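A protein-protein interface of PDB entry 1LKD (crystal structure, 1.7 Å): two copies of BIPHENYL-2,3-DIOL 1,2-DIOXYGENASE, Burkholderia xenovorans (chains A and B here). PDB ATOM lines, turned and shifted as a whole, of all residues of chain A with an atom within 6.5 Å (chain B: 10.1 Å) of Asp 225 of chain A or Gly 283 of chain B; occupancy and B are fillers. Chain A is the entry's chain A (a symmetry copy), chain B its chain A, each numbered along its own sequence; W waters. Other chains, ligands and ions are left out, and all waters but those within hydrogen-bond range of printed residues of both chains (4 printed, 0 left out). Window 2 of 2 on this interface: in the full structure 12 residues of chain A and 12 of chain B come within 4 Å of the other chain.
Among the printed residues, merely in contact across the chains: Gly 221 of chain A with Trp 282 of chain B (3.5 Å), Phe 222 of chain A with Met 281 of chain B (3.4 Å), Phe 222 of chain A with Trp 282 of chain B (3.95 Å) and Asp 225 of chain A with Trp 282 of chain B (3.2 Å).
Of the 13 printed residues of chain A, 4 touch a printed residue of chain B.
Hydrophobic or aromatic side chains of chain B within 4 Å of the printed part of chain A: Met 281 and Trp 282.
The backbone carbonyl oxygen (O) of Arg 239 of chain B is in hydrogen-bond range of the backbone NH (N) of Met 281 of chain B (2.7 Å).
OG1 of Thr 236 of chain B lies within hydrogen-bond range of N of Lys 285 of chain B (2.9 Å).
N of Arg 239 of chain B lies within hydrogen-bond range of O of Trp 282 of chain B, at 3.0 Å.
Water W4 bridges OD2 of Asp 225 of chain A (2.8 Å) and O of Gly 283 of chain B (2.8 Å).
Water W3 bridges O of Met 281 of chain B (2.8 Å) and OD2 of Asp 225 of chain A (2.8 Å).
Water W1 lies within hydrogen-bond range of the side-chain carboxylate of Asp 225 of chain A (2.8 Å), the backbone carbonyl oxygen of Gly 221 of chain A (3.0 Å) and the backbone NH of Gly 283 of chain B (3.3 Å).
Water W2 lies within hydrogen-bond range of the side-chain carboxylate of Asp 228 of chain A (2.9 Å) and the side-chain amino group of Lys 285 of chain B (3.0 Å).
The side-chain amino group (NZ) of Lys 285 of chain B lies within salt-bridge range of the side-chain carboxylate (OD2) of Asp 228 of chain A, at 2.9 Å.
The backbone NH of Gly 283 of chain B sits at hydrogen-bond distance from the side-chain carboxylate of Asp 225 of chain A, at 3.0 Å.
Positions printed for both chains: 224 and 248.
Of the printed residues of chain B, Gly 221 of chain A touches Trp 282 (3.5 Å).
Of the printed residues of chain B, Phe 222 of chain A touches Met 281 and Trp 282.
No residue of chain B comes within 4 Å of Ala 223 of chain A.
Asp 225 of chain A touches just these residues of chain B: Trp 282 and Gly 283.
Of the printed residues of chain B, Asp 228 of chain A touches Lys 285 (2.9 Å).
Ile 233 of chain A touches none of the printed residues of chain B.
Printed residues of chain A within 4 Å of Trp 282 of chain B: Gly 221 (3.5 Å), Phe 222 (3.95 Å) and Asp 225 (3.2 Å).
Of chain A, only Asp 225 (3.0 Å) comes within 4 Å of Gly 283 of chain B.
Printed residues of chain A within 4 Å of Lys 285 of chain B: Asp 228.
The nearest residue of chain A that does not touch Gly 283 of chain B is Gly 221 of chain A (5.0 Å).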
ATOM      1  N   VAL A 220     -36.306  34.177  20.880  1.00  0.00           N
ATOM      2  CA  VAL A 220     -34.982  34.001  20.298  1.00  0.00           C
ATOM      3  C   VAL A 220     -34.212  32.890  21.015  1.00  0.00           C
ATOM      4  O   VAL A 220     -33.628  32.020  20.371  1.00  0.00           O
ATOM      5  CB  VAL A 220     -34.162  35.308  20.377  1.00  0.00           C
ATOM      6  CG1 VAL A 220     -32.799  35.103  19.733  1.00  0.00           C
ATOM      7  CG2 VAL A 220     -34.911  36.436  19.678  1.00  0.00           C
ATOM      8  N   GLY A 221     -34.222  32.926  22.346  1.00  0.00           N
ATOM      9  CA  GLY A 221     -33.515  31.923  23.135  1.00  0.00           C
ATOM     10  C   GLY A 221     -33.938  30.488  22.866  1.00  0.00           C
ATOM     11  O   GLY A 221     -33.094  29.595  22.720  1.00  0.00           O
ATOM     12  N   PHE A 222     -35.245  30.254  22.805  1.00  0.00           N
ATOM     13  CA  PHE A 222     -35.759  28.915  22.540  1.00  0.00           C
ATOM     14  C   PHE A 222     -35.409  28.478  21.120  1.00  0.00           C
ATOM     15  O   PHE A 222     -35.011  27.337  20.901  1.00  0.00           O
ATOM     16  CB  PHE A 222     -37.279  28.870  22.729  1.00  0.00           C
ATOM     17  CG  PHE A 222     -37.714  28.821  24.172  1.00  0.00           C
ATOM     18  CD1 PHE A 222     -37.315  27.773  24.998  1.00  0.00           C
ATOM     19  CD2 PHE A 222     -38.542  29.810  24.699  1.00  0.00           C
ATOM     20  CE1 PHE A 222     -37.738  27.707  26.329  1.00  0.00           C
ATOM     21  CE2 PHE A 222     -38.971  29.755  26.029  1.00  0.00           C
ATOM     22  CZ  PHE A 222     -38.567  28.699  26.844  1.00  0.00           C
ATOM     23  N   ALA A 223     -35.558  29.385  20.158  1.00  0.00           N
ATOM     24  CA  ALA A 223     -35.246  29.057  18.770  1.00  0.00           C
ATOM     25  C   ALA A 223     -33.768  28.704  18.617  1.00  0.00           C
ATOM     26  O   ALA A 223     -33.412  27.791  17.868  1.00  0.00           O
ATOM     27  CB  ALA A 223     -35.598  30.223  17.861  1.00  0.00           C
ATOM     28  N   PHE A 224     -32.911  29.426  19.328  1.00  0.00           N
ATOM     29  CA  PHE A 224     -31.479  29.173  19.267  1.00  0.00           C
ATOM     30  C   PHE A 224     -31.225  27.712  19.629  1.00  0.00           C
ATOM     31  O   PHE A 224     -30.505  27.001  18.919  1.00  0.00           O
ATOM     32  CB  PHE A 224     -30.733  30.110  20.233  1.00  0.00           C
ATOM     33  CG  PHE A 224     -29.228  29.978  20.182  1.00  0.00           C
ATOM     34  CD1 PHE A 224     -28.588  28.891  20.771  1.00  0.00           C
ATOM     35  CD2 PHE A 224     -28.452  30.942  19.542  1.00  0.00           C
ATOM     36  CE1 PHE A 224     -27.195  28.764  20.725  1.00  0.00           C
ATOM     37  CE2 PHE A 224     -27.057  30.825  19.489  1.00  0.00           C
ATOM     38  CZ  PHE A 224     -26.431  29.730  20.083  1.00  0.00           C
ATOM     39  N   ASP A 225     -31.836  27.255  20.720  1.00  0.00           N
ATOM     40  CA  ASP A 225     -31.652  25.872  21.156  1.00  0.00           C
ATOM     41  C   ASP A 225     -32.213  24.843  20.176  1.00  0.00           C
ATOM     42  O   ASP A 225     -31.623  23.776  19.993  1.00  0.00           O
ATOM     43  CB  ASP A 225     -32.271  25.662  22.541  1.00  0.00           C
ATOM     44  CG  ASP A 225     -31.352  26.118  23.669  1.00  0.00           C
ATOM     45  OD1 ASP A 225     -30.297  26.720  23.378  1.00  0.00           O
ATOM     46  OD2 ASP A 225     -31.686  25.879  24.845  1.00  0.00           O
ATOM     47  N   ARG A 226     -33.345  25.150  19.547  1.00  0.00           N
ATOM     48  CA  ARG A 226     -33.928  24.209  18.595  1.00  0.00           C
ATOM     49  C   ARG A 226     -32.998  24.052  17.394  1.00  0.00           C
ATOM     50  O   ARG A 226     -32.831  22.954  16.862  1.00  0.00           O
ATOM     51  CB  ARG A 226     -35.311  24.682  18.130  1.00  0.00           C
ATOM     52  CG  ARG A 226     -36.371  24.714  19.229  1.00  0.00           C
ATOM     53  CD  ARG A 226     -37.777  24.837  18.635  1.00  0.00           C
ATOM     54  NE  ARG A 226     -37.993  26.097  17.928  1.00  0.00           N
ATOM     55  CZ  ARG A 226     -38.395  27.230  18.502  1.00  0.00           C
ATOM     56  NH1 ARG A 226     -38.635  27.273  19.807  1.00  0.00           N
ATOM     57  NH2 ARG A 226     -38.566  28.325  17.770  1.00  0.00           N
ATOM     58  N   VAL A 227     -32.385  25.155  16.980  1.00  0.00           N
ATOM     59  CA  VAL A 227     -31.469  25.151  15.846  1.00  0.00           C
ATOM     60  C   VAL A 227     -30.130  24.526  16.225  1.00  0.00           C
ATOM     61  O   VAL A 227     -29.525  23.794  15.436  1.00  0.00           O
ATOM     62  CB  VAL A 227     -31.222  26.592  15.338  1.00  0.00           C
ATOM     63  CG1 VAL A 227     -30.186  26.590  14.218  1.00  0.00           C
ATOM     64  CG2 VAL A 227     -32.534  27.197  14.854  1.00  0.00           C
ATOM     65  N   ASP A 228     -29.676  24.821  17.438  1.00  0.00           N
ATOM     66  CA  ASP A 228     -28.402  24.316  17.930  1.00  0.00           C
ATOM     67  C   ASP A 228     -28.428  22.799  18.076  1.00  0.00           C
ATOM     68  O   ASP A 228     -27.403  22.132  17.908  1.00  0.00           O
ATOM     69  CB  ASP A 228     -28.081  24.988  19.268  1.00  0.00           C
ATOM     70  CG  ASP A 228     -26.646  24.778  19.705  1.00  0.00           C
ATOM     71  OD1 ASP A 228     -25.734  24.842  18.852  1.00  0.00           O
ATOM     72  OD2 ASP A 228     -26.429  24.570  20.916  1.00  0.00           O
ATOM     73  N   ALA A 229     -29.603  22.251  18.373  1.00  0.00           N
ATOM     74  CA  ALA A 229     -29.742  20.806  18.528  1.00  0.00           C
ATOM     75  C   ALA A 229     -29.318  20.079  17.255  1.00  0.00           C
ATOM     76  O   ALA A 229     -28.845  18.942  17.311  1.00  0.00           O
ATOM     77  CB  ALA A 229     -31.183  20.451  18.873  1.00  0.00           C
ATOM     78  N   ASP A 230     -29.484  20.734  16.111  1.00  0.00           N
ATOM     79  CA  ASP A 230     -29.112  20.135  14.832  1.00  0.00           C
ATOM     80  C   ASP A 230     -27.773  20.648  14.305  1.00  0.00           C
ATOM     81  O   ASP A 230     -27.402  20.371  13.163  1.00  0.00           O
ATOM     82  CB  ASP A 230     -30.209  20.385  13.797  1.00  0.00           C
ATOM     83  CG  ASP A 230     -31.464  19.578  14.076  1.00  0.00           C
ATOM     84  OD1 ASP A 230     -31.548  18.969  15.164  1.00  0.00           O
ATOM     85  OD2 ASP A 230     -32.367  19.555  13.213  1.00  0.00           O
ATOM     86  N   ILE A 233     -26.289  26.377  14.089  1.00  0.00           N
ATOM     87  CA  ILE A 233     -25.946  27.733  14.508  1.00  0.00           C
ATOM     88  C   ILE A 233     -24.662  28.191  13.821  1.00  0.00           C
ATOM     89  O   ILE A 233     -23.692  27.440  13.746  1.00  0.00           O
ATOM     90  CB  ILE A 233     -25.736  27.813  16.039  1.00  0.00           C
ATOM     91  CG1 ILE A 233     -27.053  27.528  16.764  1.00  0.00           C
ATOM     92  CG2 ILE A 233     -25.188  29.186  16.426  1.00  0.00           C
ATOM     93  CD1 ILE A 233     -28.126  28.596  16.570  1.00  0.00           C
ATOM     94  N   PHE A 248     -29.240  35.837  16.543  1.00  0.00           N
ATOM     95  CA  PHE A 248     -28.261  34.793  16.277  1.00  0.00           C
ATOM     96  C   PHE A 248     -28.466  34.466  14.812  1.00  0.00           C
ATOM     97  O   PHE A 248     -29.477  34.864  14.220  1.00  0.00           O
ATOM     98  CB  PHE A 248     -28.479  33.547  17.154  1.00  0.00           C
ATOM     99  CG  PHE A 248     -29.714  32.752  16.818  1.00  0.00           C
ATOM    100  CD1 PHE A 248     -29.681  31.755  15.841  1.00  0.00           C
ATOM    101  CD2 PHE A 248     -30.901  32.975  17.507  1.00  0.00           C
ATOM    102  CE1 PHE A 248     -30.819  30.991  15.558  1.00  0.00           C
ATOM    103  CE2 PHE A 248     -32.043  32.219  17.234  1.00  0.00           C
ATOM    104  CZ  PHE A 248     -32.001  31.222  16.256  1.00  0.00           C
ATOM    105  N   PHE B 224     -19.933  39.291  29.286  1.00  0.00           N
ATOM    106  CA  PHE B 224     -19.688  37.974  28.717  1.00  0.00           C
ATOM    107  C   PHE B 224     -18.470  38.055  27.802  1.00  0.00           C
ATOM    108  O   PHE B 224     -17.552  37.232  27.898  1.00  0.00           O
ATOM    109  CB  PHE B 224     -20.924  37.495  27.936  1.00  0.00           C
ATOM    110  CG  PHE B 224     -20.796  36.098  27.373  1.00  0.00           C
ATOM    111  CD1 PHE B 224     -20.013  35.851  26.250  1.00  0.00           C
ATOM    112  CD2 PHE B 224     -21.460  35.030  27.972  1.00  0.00           C
ATOM    113  CE1 PHE B 224     -19.890  34.559  25.727  1.00  0.00           C
ATOM    114  CE2 PHE B 224     -21.344  33.731  27.458  1.00  0.00           C
ATOM    115  CZ  PHE B 224     -20.554  33.500  26.332  1.00  0.00           C
ATOM    116  N   THR B 234     -17.768  29.538  31.387  1.00  0.00           N
ATOM    117  CA  THR B 234     -18.038  28.139  31.704  1.00  0.00           C
ATOM    118  C   THR B 234     -19.417  27.727  31.200  1.00  0.00           C
ATOM    119  O   THR B 234     -19.707  26.539  31.066  1.00  0.00           O
ATOM    120  CB  THR B 234     -17.949  27.870  33.219  1.00  0.00           C
ATOM    121  OG1 THR B 234     -18.864  28.722  33.917  1.00  0.00           O
ATOM    122  CG2 THR B 234     -16.534  28.130  33.719  1.00  0.00           C
ATOM    123  N   SER B 235     -20.261  28.712  30.906  1.00  0.00           N
ATOM    124  CA  SER B 235     -21.604  28.440  30.404  1.00  0.00           C
ATOM    125  C   SER B 235     -22.070  29.577  29.496  1.00  0.00           C
ATOM    126  O   SER B 235     -21.826  30.748  29.782  1.00  0.00           O
ATOM    127  CB  SER B 235     -22.575  28.278  31.576  1.00  0.00           C
ATOM    128  OG  SER B 235     -23.856  27.876  31.131  1.00  0.00           O
ATOM    129  N   THR B 236     -22.724  29.230  28.393  1.00  0.00           N
ATOM    130  CA  THR B 236     -23.221  30.239  27.468  1.00  0.00           C
ATOM    131  C   THR B 236     -24.415  30.949  28.101  1.00  0.00           C
ATOM    132  O   THR B 236     -24.928  30.519  29.133  1.00  0.00           O
ATOM    133  CB  THR B 236     -23.689  29.607  26.139  1.00  0.00           C
ATOM    134  OG1 THR B 236     -24.791  28.724  26.390  1.00  0.00           O
ATOM    135  CG2 THR B 236     -22.545  28.819  25.487  1.00  0.00           C
ATOM    136  N   LEU B 237     -24.851  32.038  27.482  1.00  0.00           N
ATOM    137  CA  LEU B 237     -26.002  32.780  27.987  1.00  0.00           C
ATOM    138  C   LEU B 237     -27.236  31.877  27.994  1.00  0.00           C
ATOM    139  O   LEU B 237     -27.448  31.097  27.066  1.00  0.00           O
ATOM    140  CB  LEU B 237     -26.278  33.995  27.105  1.00  0.00           C
ATOM    141  CG  LEU B 237     -25.267  35.141  27.103  1.00  0.00           C
ATOM    142  CD1 LEU B 237     -25.630  36.122  25.999  1.00  0.00           C
ATOM    143  CD2 LEU B 237     -25.264  35.842  28.462  1.00  0.00           C
ATOM    144  N   GLY B 238     -28.043  31.986  29.044  1.00  0.00           N
ATOM    145  CA  GLY B 238     -29.254  31.188  29.135  1.00  0.00           C
ATOM    146  C   GLY B 238     -30.202  31.799  30.150  1.00  0.00           C
ATOM    147  O   GLY B 238     -29.858  32.782  30.806  1.00  0.00           O
ATOM    148  N   ARG B 239     -31.404  31.244  30.268  1.00  0.00           N
ATOM    149  CA  ARG B 239     -32.363  31.742  31.247  1.00  0.00           C
ATOM    150  C   ARG B 239     -32.788  30.575  32.118  1.00  0.00           C
ATOM    151  O   ARG B 239     -33.099  29.494  31.615  1.00  0.00           O
ATOM    152  CB  ARG B 239     -33.612  32.350  30.587  1.00  0.00           C
ATOM    153  CG  ARG B 239     -34.481  33.093  31.615  1.00  0.00           C
ATOM    154  CD  ARG B 239     -35.901  33.380  31.135  1.00  0.00           C
ATOM    155  NE  ARG B 239     -36.016  34.420  30.114  1.00  0.00           N
ATOM    156  CZ  ARG B 239     -36.083  35.729  30.351  1.00  0.00           C
ATOM    157  NH1 ARG B 239     -36.033  36.203  31.589  1.00  0.00           N
ATOM    158  NH2 ARG B 239     -36.246  36.571  29.339  1.00  0.00           N
ATOM    159  N   HIS B 240     -32.804  30.792  33.427  1.00  0.00           N
ATOM    160  CA  HIS B 240     -33.186  29.740  34.357  1.00  0.00           C
ATOM    161  C   HIS B 240     -34.681  29.467  34.385  1.00  0.00           C
ATOM    162  O   HIS B 240     -35.496  30.355  34.168  1.00  0.00           O
ATOM    163  CB  HIS B 240     -32.718  30.090  35.765  1.00  0.00           C
ATOM    164  CG  HIS B 240     -31.239  30.001  35.941  1.00  0.00           C
ATOM    165  ND1 HIS B 240     -30.540  28.828  35.753  1.00  0.00           N
ATOM    166  CD2 HIS B 240     -30.325  30.935  36.292  1.00  0.00           C
ATOM    167  CE1 HIS B 240     -29.257  29.044  35.982  1.00  0.00           C
ATOM    168  NE2 HIS B 240     -29.100  30.313  36.312  1.00  0.00           N
ATOM    169  N   THR B 241     -35.027  28.219  34.674  1.00  0.00           N
ATOM    170  CA  THR B 241     -36.417  27.802  34.746  1.00  0.00           C
ATOM    171  C   THR B 241     -37.133  28.328  35.987  1.00  0.00           C
ATOM    172  O   THR B 241     -38.335  28.607  35.940  1.00  0.00           O
ATOM    173  CB  THR B 241     -36.523  26.277  34.792  1.00  0.00           C
ATOM    174  OG1 THR B 241     -35.654  25.785  35.819  1.00  0.00           O
ATOM    175  CG2 THR B 241     -36.139  25.662  33.452  1.00  0.00           C
ATOM    176  N   MET B 245     -33.852  34.181  35.474  1.00  0.00           N
ATOM    177  CA  MET B 245     -32.730  35.094  35.306  1.00  0.00           C
ATOM    178  C   MET B 245     -31.982  34.729  34.022  1.00  0.00           C
ATOM    179  O   MET B 245     -31.802  33.543  33.720  1.00  0.00           O
ATOM    180  CB  MET B 245     -31.766  34.959  36.491  1.00  0.00           C
ATOM    181  CG  MET B 245     -30.573  35.905  36.448  1.00  0.00           C
ATOM    182  SD  MET B 245     -30.931  37.482  37.254  1.00  0.00           S
ATOM    183  CE  MET B 245     -30.581  37.057  38.966  1.00  0.00           C
ATOM    184  N   VAL B 246     -31.570  35.741  33.261  1.00  0.00           N
ATOM    185  CA  VAL B 246     -30.785  35.522  32.042  1.00  0.00           C
ATOM    186  C   VAL B 246     -29.353  35.747  32.518  1.00  0.00           C
ATOM    187  O   VAL B 246     -29.029  36.825  33.019  1.00  0.00           O
ATOM    188  CB  VAL B 246     -31.122  36.552  30.942  1.00  0.00           C
ATOM    189  CG1 VAL B 246     -30.154  36.403  29.774  1.00  0.00           C
ATOM    190  CG2 VAL B 246     -32.550  36.340  30.454  1.00  0.00           C
ATOM    191  N   SER B 247     -28.493  34.746  32.358  1.00  0.00           N
ATOM    192  CA  SER B 247     -27.131  34.864  32.855  1.00  0.00           C
ATOM    193  C   SER B 247     -26.141  33.954  32.149  1.00  0.00           C
ATOM    194  O   SER B 247     -26.504  33.168  31.281  1.00  0.00           O
ATOM    195  CB  SER B 247     -27.116  34.476  34.330  1.00  0.00           C
ATOM    196  OG  SER B 247     -27.459  33.092  34.455  1.00  0.00           O
ATOM    197  N   PHE B 248     -24.881  34.077  32.550  1.00  0.00           N
ATOM    198  CA  PHE B 248     -23.823  33.212  32.051  1.00  0.00           C
ATOM    199  C   PHE B 248     -22.972  32.934  33.274  1.00  0.00           C
ATOM    200  O   PHE B 248     -23.112  33.614  34.298  1.00  0.00           O
ATOM    201  CB  PHE B 248     -22.990  33.882  30.943  1.00  0.00           C
ATOM    202  CG  PHE B 248     -22.116  35.015  31.415  1.00  0.00           C
ATOM    203  CD1 PHE B 248     -20.828  34.775  31.896  1.00  0.00           C
ATOM    204  CD2 PHE B 248     -22.568  36.328  31.342  1.00  0.00           C
ATOM    205  CE1 PHE B 248     -20.002  35.832  32.296  1.00  0.00           C
ATOM    206  CE2 PHE B 248     -21.755  37.392  31.738  1.00  0.00           C
ATOM    207  CZ  PHE B 248     -20.466  37.142  32.216  1.00  0.00           C
ATOM    208  N   TYR B 249     -22.123  31.919  33.188  1.00  0.00           N
ATOM    209  CA  TYR B 249     -21.243  31.575  34.293  1.00  0.00           C
ATOM    210  C   TYR B 249     -19.800  31.666  33.829  1.00  0.00           C
ATOM    211  O   TYR B 249     -19.501  31.467  32.650  1.00  0.00           O
ATOM    212  CB  TYR B 249     -21.510  30.157  34.793  1.00  0.00           C
ATOM    213  CG  TYR B 249     -22.874  29.945  35.410  1.00  0.00           C
ATOM    214  CD1 TYR B 249     -24.010  29.819  34.614  1.00  0.00           C
ATOM    215  CD2 TYR B 249     -23.019  29.833  36.791  1.00  0.00           C
ATOM    216  CE1 TYR B 249     -25.261  29.577  35.183  1.00  0.00           C
ATOM    217  CE2 TYR B 249     -24.258  29.595  37.369  1.00  0.00           C
ATOM    218  CZ  TYR B 249     -25.373  29.464  36.557  1.00  0.00           C
ATOM    219  OH  TYR B 249     -26.589  29.189  37.129  1.00  0.00           O
ATOM    220  N   SER B 278     -35.142  20.523  35.084  1.00  0.00           N
ATOM    221  CA  SER B 278     -34.089  21.193  34.329  1.00  0.00           C
ATOM    222  C   SER B 278     -33.856  22.557  34.967  1.00  0.00           C
ATOM    223  O   SER B 278     -34.795  23.185  35.458  1.00  0.00           O
ATOM    224  CB  SER B 278     -34.498  21.381  32.868  1.00  0.00           C
ATOM    225  OG  SER B 278     -33.536  22.170  32.186  1.00  0.00           O
ATOM    226  N   PRO B 279     -32.599  23.031  34.977  1.00  0.00           N
ATOM    227  CA  PRO B 279     -32.308  24.338  35.575  1.00  0.00           C
ATOM    228  C   PRO B 279     -32.363  25.489  34.575  1.00  0.00           C
ATOM    229  O   PRO B 279     -32.338  26.658  34.969  1.00  0.00           O
ATOM    230  CB  PRO B 279     -30.907  24.141  36.135  1.00  0.00           C
ATOM    231  CG  PRO B 279     -30.269  23.321  35.061  1.00  0.00           C
ATOM    232  CD  PRO B 279     -31.351  22.286  34.724  1.00  0.00           C
ATOM    233  N   SER B 280     -32.447  25.164  33.286  1.00  0.00           N
ATOM    234  CA  SER B 280     -32.472  26.194  32.252  1.00  0.00           C
ATOM    235  C   SER B 280     -33.554  26.024  31.187  1.00  0.00           C
ATOM    236  O   SER B 280     -33.744  24.931  30.649  1.00  0.00           O
ATOM    237  CB  SER B 280     -31.102  26.262  31.566  1.00  0.00           C
ATOM    238  OG  SER B 280     -30.070  26.456  32.519  1.00  0.00           O
ATOM    239  N   MET B 281     -34.262  27.113  30.897  1.00  0.00           N
ATOM    240  CA  MET B 281     -35.301  27.116  29.868  1.00  0.00           C
ATOM    241  C   MET B 281     -34.602  26.988  28.530  1.00  0.00           C
ATOM    242  O   MET B 281     -35.018  26.228  27.660  1.00  0.00           O
ATOM    243  CB  MET B 281     -36.047  28.444  29.854  1.00  0.00           C
ATOM    244  CG  MET B 281     -37.201  28.556  30.776  1.00  0.00           C
ATOM    245  SD  MET B 281     -37.895  30.189  30.504  1.00  0.00           S
ATOM    246  CE  MET B 281     -37.820  30.809  32.112  1.00  0.00           C
ATOM    247  N   TRP B 282     -33.558  27.793  28.360  1.00  0.00           N
ATOM    248  CA  TRP B 282     -32.763  27.776  27.145  1.00  0.00           C
ATOM    249  C   TRP B 282     -31.354  28.232  27.478  1.00  0.00           C
ATOM    250  O   TRP B 282     -31.121  28.858  28.518  1.00  0.00           O
ATOM    251  CB  TRP B 282     -33.371  28.673  26.045  1.00  0.00           C
ATOM    252  CG  TRP B 282     -33.727  30.088  26.450  1.00  0.00           C
ATOM    253  CD1 TRP B 282     -34.960  30.548  26.823  1.00  0.00           C
ATOM    254  CD2 TRP B 282     -32.851  31.228  26.479  1.00  0.00           C
ATOM    255  NE1 TRP B 282     -34.908  31.899  27.077  1.00  0.00           N
ATOM    256  CE2 TRP B 282     -33.628  32.341  26.877  1.00  0.00           C
ATOM    257  CE3 TRP B 282     -31.489  31.415  26.207  1.00  0.00           C
ATOM    258  CZ2 TRP B 282     -33.088  33.627  27.010  1.00  0.00           C
ATOM    259  CZ3 TRP B 282     -30.947  32.700  26.340  1.00  0.00           C
ATOM    260  CH2 TRP B 282     -31.751  33.787  26.739  1.00  0.00           C
ATOM    261  N   GLY B 283     -30.409  27.893  26.608  1.00  0.00           N
ATOM    262  CA  GLY B 283     -29.034  28.292  26.832  1.00  0.00           C
ATOM    263  C   GLY B 283     -28.346  27.589  27.988  1.00  0.00           C
ATOM    264  O   GLY B 283     -28.728  26.484  28.383  1.00  0.00           O
ATOM    265  N   HIS B 284     -27.327  28.247  28.533  1.00  0.00           N
ATOM    266  CA  HIS B 284     -26.540  27.705  29.636  1.00  0.00           C
ATOM    267  C   HIS B 284     -25.870  26.403  29.220  1.00  0.00           C
ATOM    268  O   HIS B 284     -25.833  25.431  29.975  1.00  0.00           O
ATOM    269  CB  HIS B 284     -27.417  27.489  30.871  1.00  0.00           C
ATOM    270  CG  HIS B 284     -27.757  28.756  31.592  1.00  0.00           C
ATOM    271  ND1 HIS B 284     -28.898  28.898  32.353  1.00  0.00           N
ATOM    272  CD2 HIS B 284     -27.095  29.936  31.683  1.00  0.00           C
ATOM    273  CE1 HIS B 284     -28.925  30.110  32.879  1.00  0.00           C
ATOM    274  NE2 HIS B 284     -27.842  30.759  32.490  1.00  0.00           N
ATOM    275  N   LYS B 285     -25.348  26.400  28.002  1.00  0.00           N
ATOM    276  CA  LYS B 285     -24.655  25.237  27.476  1.00  0.00           C
ATOM    277  C   LYS B 285     -23.264  25.231  28.096  1.00  0.00           C
ATOM    278  O   LYS B 285     -22.580  26.260  28.116  1.00  0.00           O
ATOM    279  CB  LYS B 285     -24.536  25.329  25.954  1.00  0.00           C
ATOM    280  CG  LYS B 285     -23.898  24.105  25.314  1.00  0.00           C
ATOM    281  CD  LYS B 285     -23.274  24.429  23.958  1.00  0.00           C
ATOM    282  CE  LYS B 285     -24.286  24.990  22.976  1.00  0.00           C
ATOM    283  NZ  LYS B 285     -23.664  25.272  21.646  1.00  0.00           N
ATOM    284  N   SER B 286     -22.853  24.078  28.611  1.00  0.00           N
ATOM    285  CA  SER B 286     -21.539  23.951  29.224  1.00  0.00           C
ATOM    286  C   SER B 286     -20.460  24.053  28.158  1.00  0.00           C
ATOM    287  O   SER B 286     -20.534  23.386  27.127  1.00  0.00           O
ATOM    288  CB  SER B 286     -21.415  22.609  29.944  1.00  0.00           C
ATOM    289  OG  SER B 286     -20.096  22.425  30.420  1.00  0.00           O
ATOM    290  N   VAL B 287     -19.461  24.894  28.407  1.00  0.00           N
ATOM    291  CA  VAL B 287     -18.363  25.072  27.464  1.00  0.00           C
ATOM    292  C   VAL B 287     -17.027  25.101  28.199  1.00  0.00           C
ATOM    293  O   VAL B 287     -16.226  26.022  27.938  1.00  0.00           O
ATOM    294  CB  VAL B 287     -18.526  26.383  26.655  1.00  0.00           C
ATOM    295  CG1 VAL B 287     -19.760  26.298  25.767  1.00  0.00           C
ATOM    296  CG2 VAL B 287     -18.639  27.572  27.603  1.00  0.00           C
HETATM  297  O   HOH W   1     -30.287  29.511  23.740  1.00  0.00           O
HETATM  298  O   HOH W   2     -23.325  26.408  18.884  1.00  0.00           O
HETATM  299  O   HOH W   3     -34.461  25.362  25.062  1.00  0.00           O
HETATM  300  O   HOH W   4     -30.564  24.726  27.097  1.00  0.00           O
